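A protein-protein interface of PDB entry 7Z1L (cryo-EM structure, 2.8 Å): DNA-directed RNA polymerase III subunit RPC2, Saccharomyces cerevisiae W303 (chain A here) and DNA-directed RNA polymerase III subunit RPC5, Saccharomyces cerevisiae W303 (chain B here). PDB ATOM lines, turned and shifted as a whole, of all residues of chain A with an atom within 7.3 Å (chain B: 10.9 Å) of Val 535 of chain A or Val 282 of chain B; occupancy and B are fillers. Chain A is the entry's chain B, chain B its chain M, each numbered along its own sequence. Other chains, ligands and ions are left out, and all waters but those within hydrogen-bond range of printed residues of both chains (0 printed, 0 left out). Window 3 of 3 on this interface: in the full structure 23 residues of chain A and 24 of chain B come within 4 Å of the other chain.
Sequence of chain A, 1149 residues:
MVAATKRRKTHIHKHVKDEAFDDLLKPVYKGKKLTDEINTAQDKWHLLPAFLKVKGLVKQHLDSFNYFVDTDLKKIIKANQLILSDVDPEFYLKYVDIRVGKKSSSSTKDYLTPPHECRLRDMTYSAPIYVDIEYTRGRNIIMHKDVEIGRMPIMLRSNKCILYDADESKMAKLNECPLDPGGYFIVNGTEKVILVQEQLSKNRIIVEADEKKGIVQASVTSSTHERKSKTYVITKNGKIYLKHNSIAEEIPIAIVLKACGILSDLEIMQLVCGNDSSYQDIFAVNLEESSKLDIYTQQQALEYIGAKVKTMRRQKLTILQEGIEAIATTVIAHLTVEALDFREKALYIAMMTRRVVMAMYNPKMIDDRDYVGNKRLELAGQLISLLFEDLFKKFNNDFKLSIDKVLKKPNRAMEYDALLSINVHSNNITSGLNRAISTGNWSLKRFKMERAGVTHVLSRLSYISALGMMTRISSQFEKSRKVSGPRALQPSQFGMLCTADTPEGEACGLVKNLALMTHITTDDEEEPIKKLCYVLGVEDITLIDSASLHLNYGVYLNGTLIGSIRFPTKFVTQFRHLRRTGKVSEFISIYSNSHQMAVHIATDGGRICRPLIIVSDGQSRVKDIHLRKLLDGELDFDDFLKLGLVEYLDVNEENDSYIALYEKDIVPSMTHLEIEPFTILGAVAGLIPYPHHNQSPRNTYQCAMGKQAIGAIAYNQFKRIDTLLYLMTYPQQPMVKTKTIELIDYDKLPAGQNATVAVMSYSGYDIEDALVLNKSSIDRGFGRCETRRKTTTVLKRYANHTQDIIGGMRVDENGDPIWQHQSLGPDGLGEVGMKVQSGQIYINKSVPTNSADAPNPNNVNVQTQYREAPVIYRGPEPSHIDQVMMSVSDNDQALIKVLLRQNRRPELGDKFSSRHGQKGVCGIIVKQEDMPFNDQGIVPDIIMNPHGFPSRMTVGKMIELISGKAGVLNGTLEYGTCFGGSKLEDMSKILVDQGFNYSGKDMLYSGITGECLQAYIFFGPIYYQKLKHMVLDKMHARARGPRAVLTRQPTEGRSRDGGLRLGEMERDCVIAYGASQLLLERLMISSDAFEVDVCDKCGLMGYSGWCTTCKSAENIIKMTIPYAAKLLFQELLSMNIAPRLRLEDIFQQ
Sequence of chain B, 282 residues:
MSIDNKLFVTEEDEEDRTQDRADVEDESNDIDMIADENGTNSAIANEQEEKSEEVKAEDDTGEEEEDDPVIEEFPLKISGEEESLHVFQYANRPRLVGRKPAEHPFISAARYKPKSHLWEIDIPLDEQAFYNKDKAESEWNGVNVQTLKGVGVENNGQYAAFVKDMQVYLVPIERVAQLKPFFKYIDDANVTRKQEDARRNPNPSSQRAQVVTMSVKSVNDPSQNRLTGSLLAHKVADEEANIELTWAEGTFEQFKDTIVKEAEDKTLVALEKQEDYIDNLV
Of the 15 printed residues of chain B, 3 touch a printed residue of chain A.
Hydrophobic or aromatic side chains of chain B that line the printed part of chain A: Val 282.
Of the 16 printed residues of chain A, 4 touch a printed residue of chain B.
Among the printed residues, 6 pairs touch across the chains.
CD1 of Leu 532 of chain A touches O of Val 282 of chain B, at 3.3 Å.
Val 282 of chain B touches Val 535 of chain A.
Val 282 of chain B touches Leu 578 of chain A (CG1 to CD2, 3.7 Å).
Lys 583 of chain A touches Ile 278 of chain B (CE to O, 3.7 Å).
CE of Lys 583 of chain A touches O of Asp 279 of chain B, 3.7 Å away.
Val 282 of chain B touches Lys 583 of chain A.
The backbone NH (N) of Lys 583 of chain A sits at hydrogen-bond distance from the backbone carbonyl oxygen (O) of Leu 578 of chain A (3.0 Å).
Leu 532 of chain A touches one residue of chain B.
Cys 533 of chain A touches none of the printed residues of chain B.
Val 535 of chain A touches just one residue of chain B: Val 282 (3.2 Å).
No residue of chain B comes within 4 Å of Leu 536 of chain A.
No residue of chain B comes within 4 Å of Gly 537 of chain A.
Of the printed residues of chain B, Leu 578 of chain A touches Val 282 (3.7 Å).
Lys 583 of chain A touches three residues of chain B.
Of the printed residues of chain A, Ile 278 of chain B touches Lys 583.
The nearest residue of chain A that does not touch Val 282 of chain B is Leu 536 of chain A (4.1 Å).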
ATOM      1  N   ILE A 529      26.949   2.009   7.622  1.00  0.00           N
ATOM      2  CA  ILE A 529      28.229   1.425   8.010  1.00  0.00           C
ATOM      3  C   ILE A 529      28.164   0.902   9.440  1.00  0.00           C
ATOM      4  O   ILE A 529      28.726  -0.154   9.752  1.00  0.00           O
ATOM      5  CB  ILE A 529      29.361   2.451   7.827  1.00  0.00           C
ATOM      6  CG1 ILE A 529      29.364   2.986   6.397  1.00  0.00           C
ATOM      7  CG2 ILE A 529      30.708   1.828   8.141  1.00  0.00           C
ATOM      8  CD1 ILE A 529      29.536   1.913   5.349  1.00  0.00           C
ATOM      9  N   LYS A 530      27.465   1.617  10.324  1.00  0.00           N
ATOM     10  CA  LYS A 530      27.297   1.161  11.702  1.00  0.00           C
ATOM     11  C   LYS A 530      26.516  -0.148  11.759  1.00  0.00           C
ATOM     12  O   LYS A 530      26.892  -1.088  12.478  1.00  0.00           O
ATOM     13  CB  LYS A 530      26.596   2.252  12.512  1.00  0.00           C
ATOM     14  CG  LYS A 530      26.380   1.939  13.976  1.00  0.00           C
ATOM     15  CD  LYS A 530      26.668   3.159  14.833  1.00  0.00           C
ATOM     16  CE  LYS A 530      26.605   2.830  16.315  1.00  0.00           C
ATOM     17  NZ  LYS A 530      25.205   2.731  16.809  1.00  0.00           N
ATOM     18  N   LYS A 531      25.428  -0.235  10.989  1.00  0.00           N
ATOM     19  CA  LYS A 531      24.648  -1.468  10.953  1.00  0.00           C
ATOM     20  C   LYS A 531      25.445  -2.610  10.335  1.00  0.00           C
ATOM     21  O   LYS A 531      25.335  -3.761  10.774  1.00  0.00           O
ATOM     22  CB  LYS A 531      23.344  -1.241  10.191  1.00  0.00           C
ATOM     23  CG  LYS A 531      22.388  -0.298  10.893  1.00  0.00           C
ATOM     24  CD  LYS A 531      21.089  -0.149  10.125  1.00  0.00           C
ATOM     25  CE  LYS A 531      20.173   0.860  10.795  1.00  0.00           C
ATOM     26  NZ  LYS A 531      19.687   0.369  12.115  1.00  0.00           N
ATOM     27  N   LEU A 532      26.258  -2.311   9.318  1.00  0.00           N
ATOM     28  CA  LEU A 532      27.111  -3.332   8.720  1.00  0.00           C
ATOM     29  C   LEU A 532      28.155  -3.830   9.711  1.00  0.00           C
ATOM     30  O   LEU A 532      28.486  -5.021   9.730  1.00  0.00           O
ATOM     31  CB  LEU A 532      27.784  -2.776   7.469  1.00  0.00           C
ATOM     32  CG  LEU A 532      28.458  -3.799   6.561  1.00  0.00           C
ATOM     33  CD1 LEU A 532      27.434  -4.432   5.642  1.00  0.00           C
ATOM     34  CD2 LEU A 532      29.561  -3.135   5.766  1.00  0.00           C
ATOM     35  N   CYS A 533      28.695  -2.925  10.531  1.00  0.00           N
ATOM     36  CA  CYS A 533      29.615  -3.329  11.590  1.00  0.00           C
ATOM     37  C   CYS A 533      28.933  -4.258  12.579  1.00  0.00           C
ATOM     38  O   CYS A 533      29.508  -5.275  12.985  1.00  0.00           O
ATOM     39  CB  CYS A 533      30.150  -2.101  12.321  1.00  0.00           C
ATOM     40  SG  CYS A 533      31.267  -1.092  11.360  1.00  0.00           S
ATOM     41  N   TYR A 534      27.704  -3.922  12.979  1.00  0.00           N
ATOM     42  CA  TYR A 534      26.979  -4.774  13.917  1.00  0.00           C
ATOM     43  C   TYR A 534      26.672  -6.137  13.308  1.00  0.00           C
ATOM     44  O   TYR A 534      26.677  -7.155  14.010  1.00  0.00           O
ATOM     45  CB  TYR A 534      25.695  -4.085  14.373  1.00  0.00           C
ATOM     46  CG  TYR A 534      25.923  -2.984  15.380  1.00  0.00           C
ATOM     47  CD1 TYR A 534      27.040  -2.993  16.202  1.00  0.00           C
ATOM     48  CD2 TYR A 534      25.024  -1.937  15.509  1.00  0.00           C
ATOM     49  CE1 TYR A 534      27.256  -1.991  17.122  1.00  0.00           C
ATOM     50  CE2 TYR A 534      25.231  -0.929  16.427  1.00  0.00           C
ATOM     51  CZ  TYR A 534      26.347  -0.962  17.232  1.00  0.00           C
ATOM     52  OH  TYR A 534      26.557   0.041  18.149  1.00  0.00           O
ATOM     53  N   VAL A 535      26.393  -6.176  12.003  1.00  0.00           N
ATOM     54  CA  VAL A 535      26.102  -7.446  11.343  1.00  0.00           C
ATOM     55  C   VAL A 535      27.359  -8.303  11.226  1.00  0.00           C
ATOM     56  O   VAL A 535      27.326  -9.512  11.480  1.00  0.00           O
ATOM     57  CB  VAL A 535      25.453  -7.194   9.969  1.00  0.00           C
ATOM     58  CG1 VAL A 535      25.438  -8.465   9.144  1.00  0.00           C
ATOM     59  CG2 VAL A 535      24.037  -6.674  10.144  1.00  0.00           C
ATOM     60  N   LEU A 536      28.493  -7.692  10.871  1.00  0.00           N
ATOM     61  CA  LEU A 536      29.708  -8.448  10.581  1.00  0.00           C
ATOM     62  C   LEU A 536      30.325  -9.107  11.809  1.00  0.00           C
ATOM     63  O   LEU A 536      31.252  -9.907  11.650  1.00  0.00           O
ATOM     64  CB  LEU A 536      30.748  -7.548   9.913  1.00  0.00           C
ATOM     65  CG  LEU A 536      30.560  -7.286   8.418  1.00  0.00           C
ATOM     66  CD1 LEU A 536      31.641  -6.362   7.897  1.00  0.00           C
ATOM     67  CD2 LEU A 536      30.552  -8.589   7.642  1.00  0.00           C
ATOM     68  N   GLY A 537      29.856  -8.794  13.012  1.00  0.00           N
ATOM     69  CA  GLY A 537      30.321  -9.506  14.185  1.00  0.00           C
ATOM     70  C   GLY A 537      30.925  -8.639  15.268  1.00  0.00           C
ATOM     71  O   GLY A 537      31.735  -9.116  16.068  1.00  0.00           O
ATOM     72  N   VAL A 538      30.542  -7.370  15.311  1.00  0.00           N
ATOM     73  CA  VAL A 538      31.024  -6.450  16.332  1.00  0.00           C
ATOM     74  C   VAL A 538      30.034  -6.453  17.488  1.00  0.00           C
ATOM     75  O   VAL A 538      28.861  -6.108  17.313  1.00  0.00           O
ATOM     76  CB  VAL A 538      31.205  -5.034  15.764  1.00  0.00           C
ATOM     77  CG1 VAL A 538      31.411  -4.030  16.883  1.00  0.00           C
ATOM     78  CG2 VAL A 538      32.367  -5.002  14.791  1.00  0.00           C
ATOM     79  N   PHE A 571      37.668  -9.360  10.101  1.00  0.00           N
ATOM     80  CA  PHE A 571      36.749  -8.238   9.941  1.00  0.00           C
ATOM     81  C   PHE A 571      37.275  -7.234   8.922  1.00  0.00           C
ATOM     82  O   PHE A 571      36.523  -6.752   8.065  1.00  0.00           O
ATOM     83  CB  PHE A 571      36.523  -7.569  11.296  1.00  0.00           C
ATOM     84  CG  PHE A 571      35.640  -6.357  11.244  1.00  0.00           C
ATOM     85  CD1 PHE A 571      34.266  -6.487  11.201  1.00  0.00           C
ATOM     86  CD2 PHE A 571      36.186  -5.084  11.269  1.00  0.00           C
ATOM     87  CE1 PHE A 571      33.453  -5.375  11.164  1.00  0.00           C
ATOM     88  CE2 PHE A 571      35.377  -3.969  11.231  1.00  0.00           C
ATOM     89  CZ  PHE A 571      34.010  -4.115  11.180  1.00  0.00           C
ATOM     90  N   GLN A 574      37.035  -8.789   5.404  1.00  0.00           N
ATOM     91  CA  GLN A 574      35.653  -8.794   4.934  1.00  0.00           C
ATOM     92  C   GLN A 574      35.192  -7.397   4.539  1.00  0.00           C
ATOM     93  O   GLN A 574      34.492  -7.227   3.532  1.00  0.00           O
ATOM     94  CB  GLN A 574      34.744  -9.378   6.012  1.00  0.00           C
ATOM     95  CG  GLN A 574      34.823 -10.889   6.130  1.00  0.00           C
ATOM     96  CD  GLN A 574      33.818 -11.450   7.112  1.00  0.00           C
ATOM     97  OE1 GLN A 574      33.128 -10.703   7.804  1.00  0.00           O
ATOM     98  NE2 GLN A 574      33.729 -12.772   7.178  1.00  0.00           N
ATOM     99  N   HIS A 577      36.735  -6.574   1.255  1.00  0.00           N
ATOM    100  CA  HIS A 577      36.051  -7.295   0.188  1.00  0.00           C
ATOM    101  C   HIS A 577      34.726  -6.632  -0.163  1.00  0.00           C
ATOM    102  O   HIS A 577      34.358  -6.545  -1.340  1.00  0.00           O
ATOM    103  CB  HIS A 577      35.833  -8.752   0.593  1.00  0.00           C
ATOM    104  CG  HIS A 577      35.084  -9.558  -0.421  1.00  0.00           C
ATOM    105  ND1 HIS A 577      35.717 -10.295  -1.397  1.00  0.00           N
ATOM    106  CD2 HIS A 577      33.757  -9.748  -0.607  1.00  0.00           C
ATOM    107  CE1 HIS A 577      34.813 -10.902  -2.144  1.00  0.00           C
ATOM    108  NE2 HIS A 577      33.614 -10.586  -1.686  1.00  0.00           N
ATOM    109  N   LEU A 578      33.993  -6.160   0.849  1.00  0.00           N
ATOM    110  CA  LEU A 578      32.747  -5.444   0.587  1.00  0.00           C
ATOM    111  C   LEU A 578      33.005  -4.131  -0.138  1.00  0.00           C
ATOM    112  O   LEU A 578      32.223  -3.729  -1.007  1.00  0.00           O
ATOM    113  CB  LEU A 578      31.999  -5.194   1.894  1.00  0.00           C
ATOM    114  CG  LEU A 578      31.237  -6.397   2.436  1.00  0.00           C
ATOM    115  CD1 LEU A 578      30.404  -6.006   3.633  1.00  0.00           C
ATOM    116  CD2 LEU A 578      30.369  -7.003   1.350  1.00  0.00           C
ATOM    117  N   LYS A 583      29.640  -2.930  -2.294  1.00  0.00           N
ATOM    118  CA  LYS A 583      28.503  -2.885  -1.385  1.00  0.00           C
ATOM    119  C   LYS A 583      28.513  -1.653  -0.493  1.00  0.00           C
ATOM    120  O   LYS A 583      27.445  -1.211  -0.056  1.00  0.00           O
ATOM    121  CB  LYS A 583      28.465  -4.150  -0.525  1.00  0.00           C
ATOM    122  CG  LYS A 583      27.559  -5.246  -1.071  1.00  0.00           C
ATOM    123  CD  LYS A 583      28.073  -5.799  -2.392  1.00  0.00           C
ATOM    124  CE  LYS A 583      27.057  -6.718  -3.043  1.00  0.00           C
ATOM    125  NZ  LYS A 583      27.479  -7.123  -4.412  1.00  0.00           N
ATOM    126  N   VAL A 584      29.689  -1.093  -0.209  1.00  0.00           N
ATOM    127  CA  VAL A 584      29.809   0.151   0.537  1.00  0.00           C
ATOM    128  C   VAL A 584      30.577   1.147  -0.320  1.00  0.00           C
ATOM    129  O   VAL A 584      31.094   0.813  -1.389  1.00  0.00           O
ATOM    130  CB  VAL A 584      30.503  -0.039   1.902  1.00  0.00           C
ATOM    131  CG1 VAL A 584      29.675  -0.941   2.792  1.00  0.00           C
ATOM    132  CG2 VAL A 584      31.895  -0.604   1.716  1.00  0.00           C
ATOM    133  N   ASN B 155      18.828  -3.408  22.264  1.00  0.00           N
ATOM    134  CA  ASN B 155      19.820  -3.992  21.373  1.00  0.00           C
ATOM    135  C   ASN B 155      19.123  -4.954  20.423  1.00  0.00           C
ATOM    136  O   ASN B 155      18.378  -5.835  20.863  1.00  0.00           O
ATOM    137  CB  ASN B 155      20.912  -4.719  22.161  1.00  0.00           C
ATOM    138  CG  ASN B 155      22.050  -3.802  22.558  1.00  0.00           C
ATOM    139  OD1 ASN B 155      22.330  -3.619  23.741  1.00  0.00           O
ATOM    140  ND2 ASN B 155      22.713  -3.220  21.566  1.00  0.00           N
ATOM    141  N   ASN B 156      19.367  -4.782  19.129  1.00  0.00           N
ATOM    142  CA  ASN B 156      18.728  -5.585  18.098  1.00  0.00           C
ATOM    143  C   ASN B 156      19.648  -6.717  17.665  1.00  0.00           C
ATOM    144  O   ASN B 156      20.853  -6.518  17.482  1.00  0.00           O
ATOM    145  CB  ASN B 156      18.356  -4.724  16.890  1.00  0.00           C
ATOM    146  CG  ASN B 156      17.156  -3.839  17.155  1.00  0.00           C
ATOM    147  OD1 ASN B 156      16.049  -4.327  17.384  1.00  0.00           O
ATOM    148  ND2 ASN B 156      17.368  -2.528  17.125  1.00  0.00           N
ATOM    149  N   GLY B 157      19.074  -7.904  17.502  1.00  0.00           N
ATOM    150  CA  GLY B 157      19.822  -9.062  17.067  1.00  0.00           C
ATOM    151  C   GLY B 157      20.337  -9.956  18.169  1.00  0.00           C
ATOM    152  O   GLY B 157      21.168 -10.830  17.894  1.00  0.00           O
ATOM    153  N   GLN B 158      19.876  -9.774  19.403  1.00  0.00           N
ATOM    154  CA  GLN B 158      20.301 -10.594  20.528  1.00  0.00           C
ATOM    155  C   GLN B 158      19.211 -11.601  20.861  1.00  0.00           C
ATOM    156  O   GLN B 158      18.053 -11.224  21.067  1.00  0.00           O
ATOM    157  CB  GLN B 158      20.608  -9.729  21.751  1.00  0.00           C
ATOM    158  CG  GLN B 158      21.503  -8.538  21.467  1.00  0.00           C
ATOM    159  CD  GLN B 158      22.896  -8.942  21.030  1.00  0.00           C
ATOM    160  OE1 GLN B 158      23.404  -9.991  21.425  1.00  0.00           O
ATOM    161  NE2 GLN B 158      23.522  -8.108  20.210  1.00  0.00           N
ATOM    162  N   GLU B 272      15.061 -16.532   0.196  1.00  0.00           N
ATOM    163  CA  GLU B 272      16.133 -15.743  -0.395  1.00  0.00           C
ATOM    164  C   GLU B 272      17.307 -16.621  -0.812  1.00  0.00           C
ATOM    165  O   GLU B 272      17.642 -17.605  -0.146  1.00  0.00           O
ATOM    166  CB  GLU B 272      16.607 -14.674   0.587  1.00  0.00           C
ATOM    167  CG  GLU B 272      17.154 -13.422  -0.080  1.00  0.00           C
ATOM    168  CD  GLU B 272      17.089 -12.206   0.821  1.00  0.00           C
ATOM    169  OE1 GLU B 272      16.039 -11.992   1.460  1.00  0.00           O
ATOM    170  OE2 GLU B 272      18.088 -11.459   0.888  1.00  0.00           O
ATOM    171  N   LYS B 273      17.932 -16.252  -1.927  1.00  0.00           N
ATOM    172  CA  LYS B 273      19.138 -16.904  -2.407  1.00  0.00           C
ATOM    173  C   LYS B 273      20.328 -16.469  -1.549  1.00  0.00           C
ATOM    174  O   LYS B 273      20.291 -15.433  -0.879  1.00  0.00           O
ATOM    175  CB  LYS B 273      19.347 -16.564  -3.890  1.00  0.00           C
ATOM    176  CG  LYS B 273      20.556 -17.190  -4.579  1.00  0.00           C
ATOM    177  CD  LYS B 273      20.383 -18.693  -4.738  1.00  0.00           C
ATOM    178  CE  LYS B 273      21.535 -19.301  -5.518  1.00  0.00           C
ATOM    179  NZ  LYS B 273      21.414 -20.782  -5.625  1.00  0.00           N
ATOM    180  N   GLN B 274      21.379 -17.294  -1.549  1.00  0.00           N
ATOM    181  CA  GLN B 274      22.575 -16.995  -0.766  1.00  0.00           C
ATOM    182  C   GLN B 274      23.223 -15.691  -1.221  1.00  0.00           C
ATOM    183  O   GLN B 274      23.651 -14.876  -0.397  1.00  0.00           O
ATOM    184  CB  GLN B 274      23.563 -18.161  -0.860  1.00  0.00           C
ATOM    185  CG  GLN B 274      24.777 -18.072   0.064  1.00  0.00           C
ATOM    186  CD  GLN B 274      25.925 -17.272  -0.524  1.00  0.00           C
ATOM    187  OE1 GLN B 274      26.101 -17.220  -1.740  1.00  0.00           O
ATOM    188  NE2 GLN B 274      26.713 -16.644   0.341  1.00  0.00           N
ATOM    189  N   GLU B 275      23.307 -15.477  -2.536  1.00  0.00           N
ATOM    190  CA  GLU B 275      23.924 -14.260  -3.048  1.00  0.00           C
ATOM    191  C   GLU B 275      23.026 -13.040  -2.877  1.00  0.00           C
ATOM    192  O   GLU B 275      23.531 -11.921  -2.724  1.00  0.00           O
ATOM    193  CB  GLU B 275      24.296 -14.437  -4.520  1.00  0.00           C
ATOM    194  CG  GLU B 275      25.496 -15.343  -4.747  1.00  0.00           C
ATOM    195  CD  GLU B 275      26.790 -14.735  -4.241  1.00  0.00           C
ATOM    196  OE1 GLU B 275      26.947 -13.500  -4.336  1.00  0.00           O
ATOM    197  OE2 GLU B 275      27.650 -15.494  -3.745  1.00  0.00           O
ATOM    198  N   ASP B 276      21.704 -13.229  -2.906  1.00  0.00           N
ATOM    199  CA  ASP B 276      20.794 -12.101  -2.727  1.00  0.00           C
ATOM    200  C   ASP B 276      20.863 -11.543  -1.312  1.00  0.00           C
ATOM    201  O   ASP B 276      20.657 -10.341  -1.110  1.00  0.00           O
ATOM    202  CB  ASP B 276      19.364 -12.521  -3.067  1.00  0.00           C
ATOM    203  CG  ASP B 276      18.566 -11.400  -3.700  1.00  0.00           C
ATOM    204  OD1 ASP B 276      18.983 -10.229  -3.581  1.00  0.00           O
ATOM    205  OD2 ASP B 276      17.520 -11.690  -4.319  1.00  0.00           O
ATOM    206  N   TYR B 277      21.132 -12.398  -0.323  1.00  0.00           N
ATOM    207  CA  TYR B 277      21.343 -11.914   1.038  1.00  0.00           C
ATOM    208  C   TYR B 277      22.608 -11.073   1.128  1.00  0.00           C
ATOM    209  O   TYR B 277      22.645 -10.063   1.840  1.00  0.00           O
ATOM    210  CB  TYR B 277      21.414 -13.090   2.010  1.00  0.00           C
ATOM    211  CG  TYR B 277      21.667 -12.685   3.442  1.00  0.00           C
ATOM    212  CD1 TYR B 277      20.837 -11.774   4.083  1.00  0.00           C
ATOM    213  CD2 TYR B 277      22.735 -13.212   4.155  1.00  0.00           C
ATOM    214  CE1 TYR B 277      21.065 -11.402   5.392  1.00  0.00           C
ATOM    215  CE2 TYR B 277      22.969 -12.845   5.464  1.00  0.00           C
ATOM    216  CZ  TYR B 277      22.131 -11.940   6.077  1.00  0.00           C
ATOM    217  OH  TYR B 277      22.360 -11.570   7.381  1.00  0.00           O
ATOM    218  N   ILE B 278      23.658 -11.478   0.411  1.00  0.00           N
ATOM    219  CA  ILE B 278      24.903 -10.727   0.407  1.00  0.00           C
ATOM    220  C   ILE B 278      24.759  -9.449  -0.418  1.00  0.00           C
ATOM    221  O   ILE B 278      25.529  -8.500  -0.237  1.00  0.00           O
ATOM    222  CB  ILE B 278      26.027 -11.650  -0.106  1.00  0.00           C
ATOM    223  CG1 ILE B 278      26.126 -12.882   0.793  1.00  0.00           C
ATOM    224  CG2 ILE B 278      27.385 -10.961  -0.105  1.00  0.00           C
ATOM    225  CD1 ILE B 278      26.456 -12.567   2.228  1.00  0.00           C
ATOM    226  N   ASP B 279      23.759  -9.392  -1.302  1.00  0.00           N
ATOM    227  CA  ASP B 279      23.574  -8.215  -2.147  1.00  0.00           C
ATOM    228  C   ASP B 279      23.221  -6.976  -1.328  1.00  0.00           C
ATOM    229  O   ASP B 279      23.706  -5.877  -1.620  1.00  0.00           O
ATOM    230  CB  ASP B 279      22.495  -8.487  -3.194  1.00  0.00           C
ATOM    231  CG  ASP B 279      22.342  -7.348  -4.180  1.00  0.00           C
ATOM    232  OD1 ASP B 279      23.277  -7.119  -4.975  1.00  0.00           O
ATOM    233  OD2 ASP B 279      21.286  -6.681  -4.162  1.00  0.00           O
ATOM    234  N   ASN B 280      22.384  -7.127  -0.303  1.00  0.00           N
ATOM    235  CA  ASN B 280      21.955  -5.993   0.506  1.00  0.00           C
ATOM    236  C   ASN B 280      22.039  -6.297   1.998  1.00  0.00           C
ATOM    237  O   ASN B 280      21.713  -7.402   2.442  1.00  0.00           O
ATOM    238  CB  ASN B 280      20.535  -5.522   0.090  1.00  0.00           C
ATOM    239  CG  ASN B 280      19.462  -6.603   0.223  1.00  0.00           C
ATOM    240  OD1 ASN B 280      19.702  -7.704   0.707  1.00  0.00           O
ATOM    241  ND2 ASN B 280      18.255  -6.272  -0.220  1.00  0.00           N
ATOM    242  N   LEU B 281      22.501  -5.300   2.756  1.00  0.00           N
ATOM    243  CA  LEU B 281      22.715  -5.372   4.206  1.00  0.00           C
ATOM    244  C   LEU B 281      23.513  -6.623   4.585  1.00  0.00           C
ATOM    245  O   LEU B 281      23.026  -7.541   5.246  1.00  0.00           O
ATOM    246  CB  LEU B 281      21.388  -5.301   4.968  1.00  0.00           C
ATOM    247  CG  LEU B 281      21.532  -4.640   6.342  1.00  0.00           C
ATOM    248  CD1 LEU B 281      22.173  -3.266   6.212  1.00  0.00           C
ATOM    249  CD2 LEU B 281      20.194  -4.532   7.049  1.00  0.00           C
ATOM    250  N   VAL B 282      24.756  -6.626   4.118  1.00  0.00           N
ATOM    251  CA  VAL B 282      25.648  -7.774   4.215  1.00  0.00           C
ATOM    252  C   VAL B 282      25.899  -8.179   5.661  1.00  0.00           C
ATOM    253  O   VAL B 282      26.798  -7.648   6.314  1.00  0.00           O
ATOM    254  CB  VAL B 282      26.981  -7.474   3.520  1.00  0.00           C
ATOM    255  CG1 VAL B 282      27.814  -8.734   3.403  1.00  0.00           C
ATOM    256  CG2 VAL B 282      26.747  -6.819   2.174  1.00  0.00           C
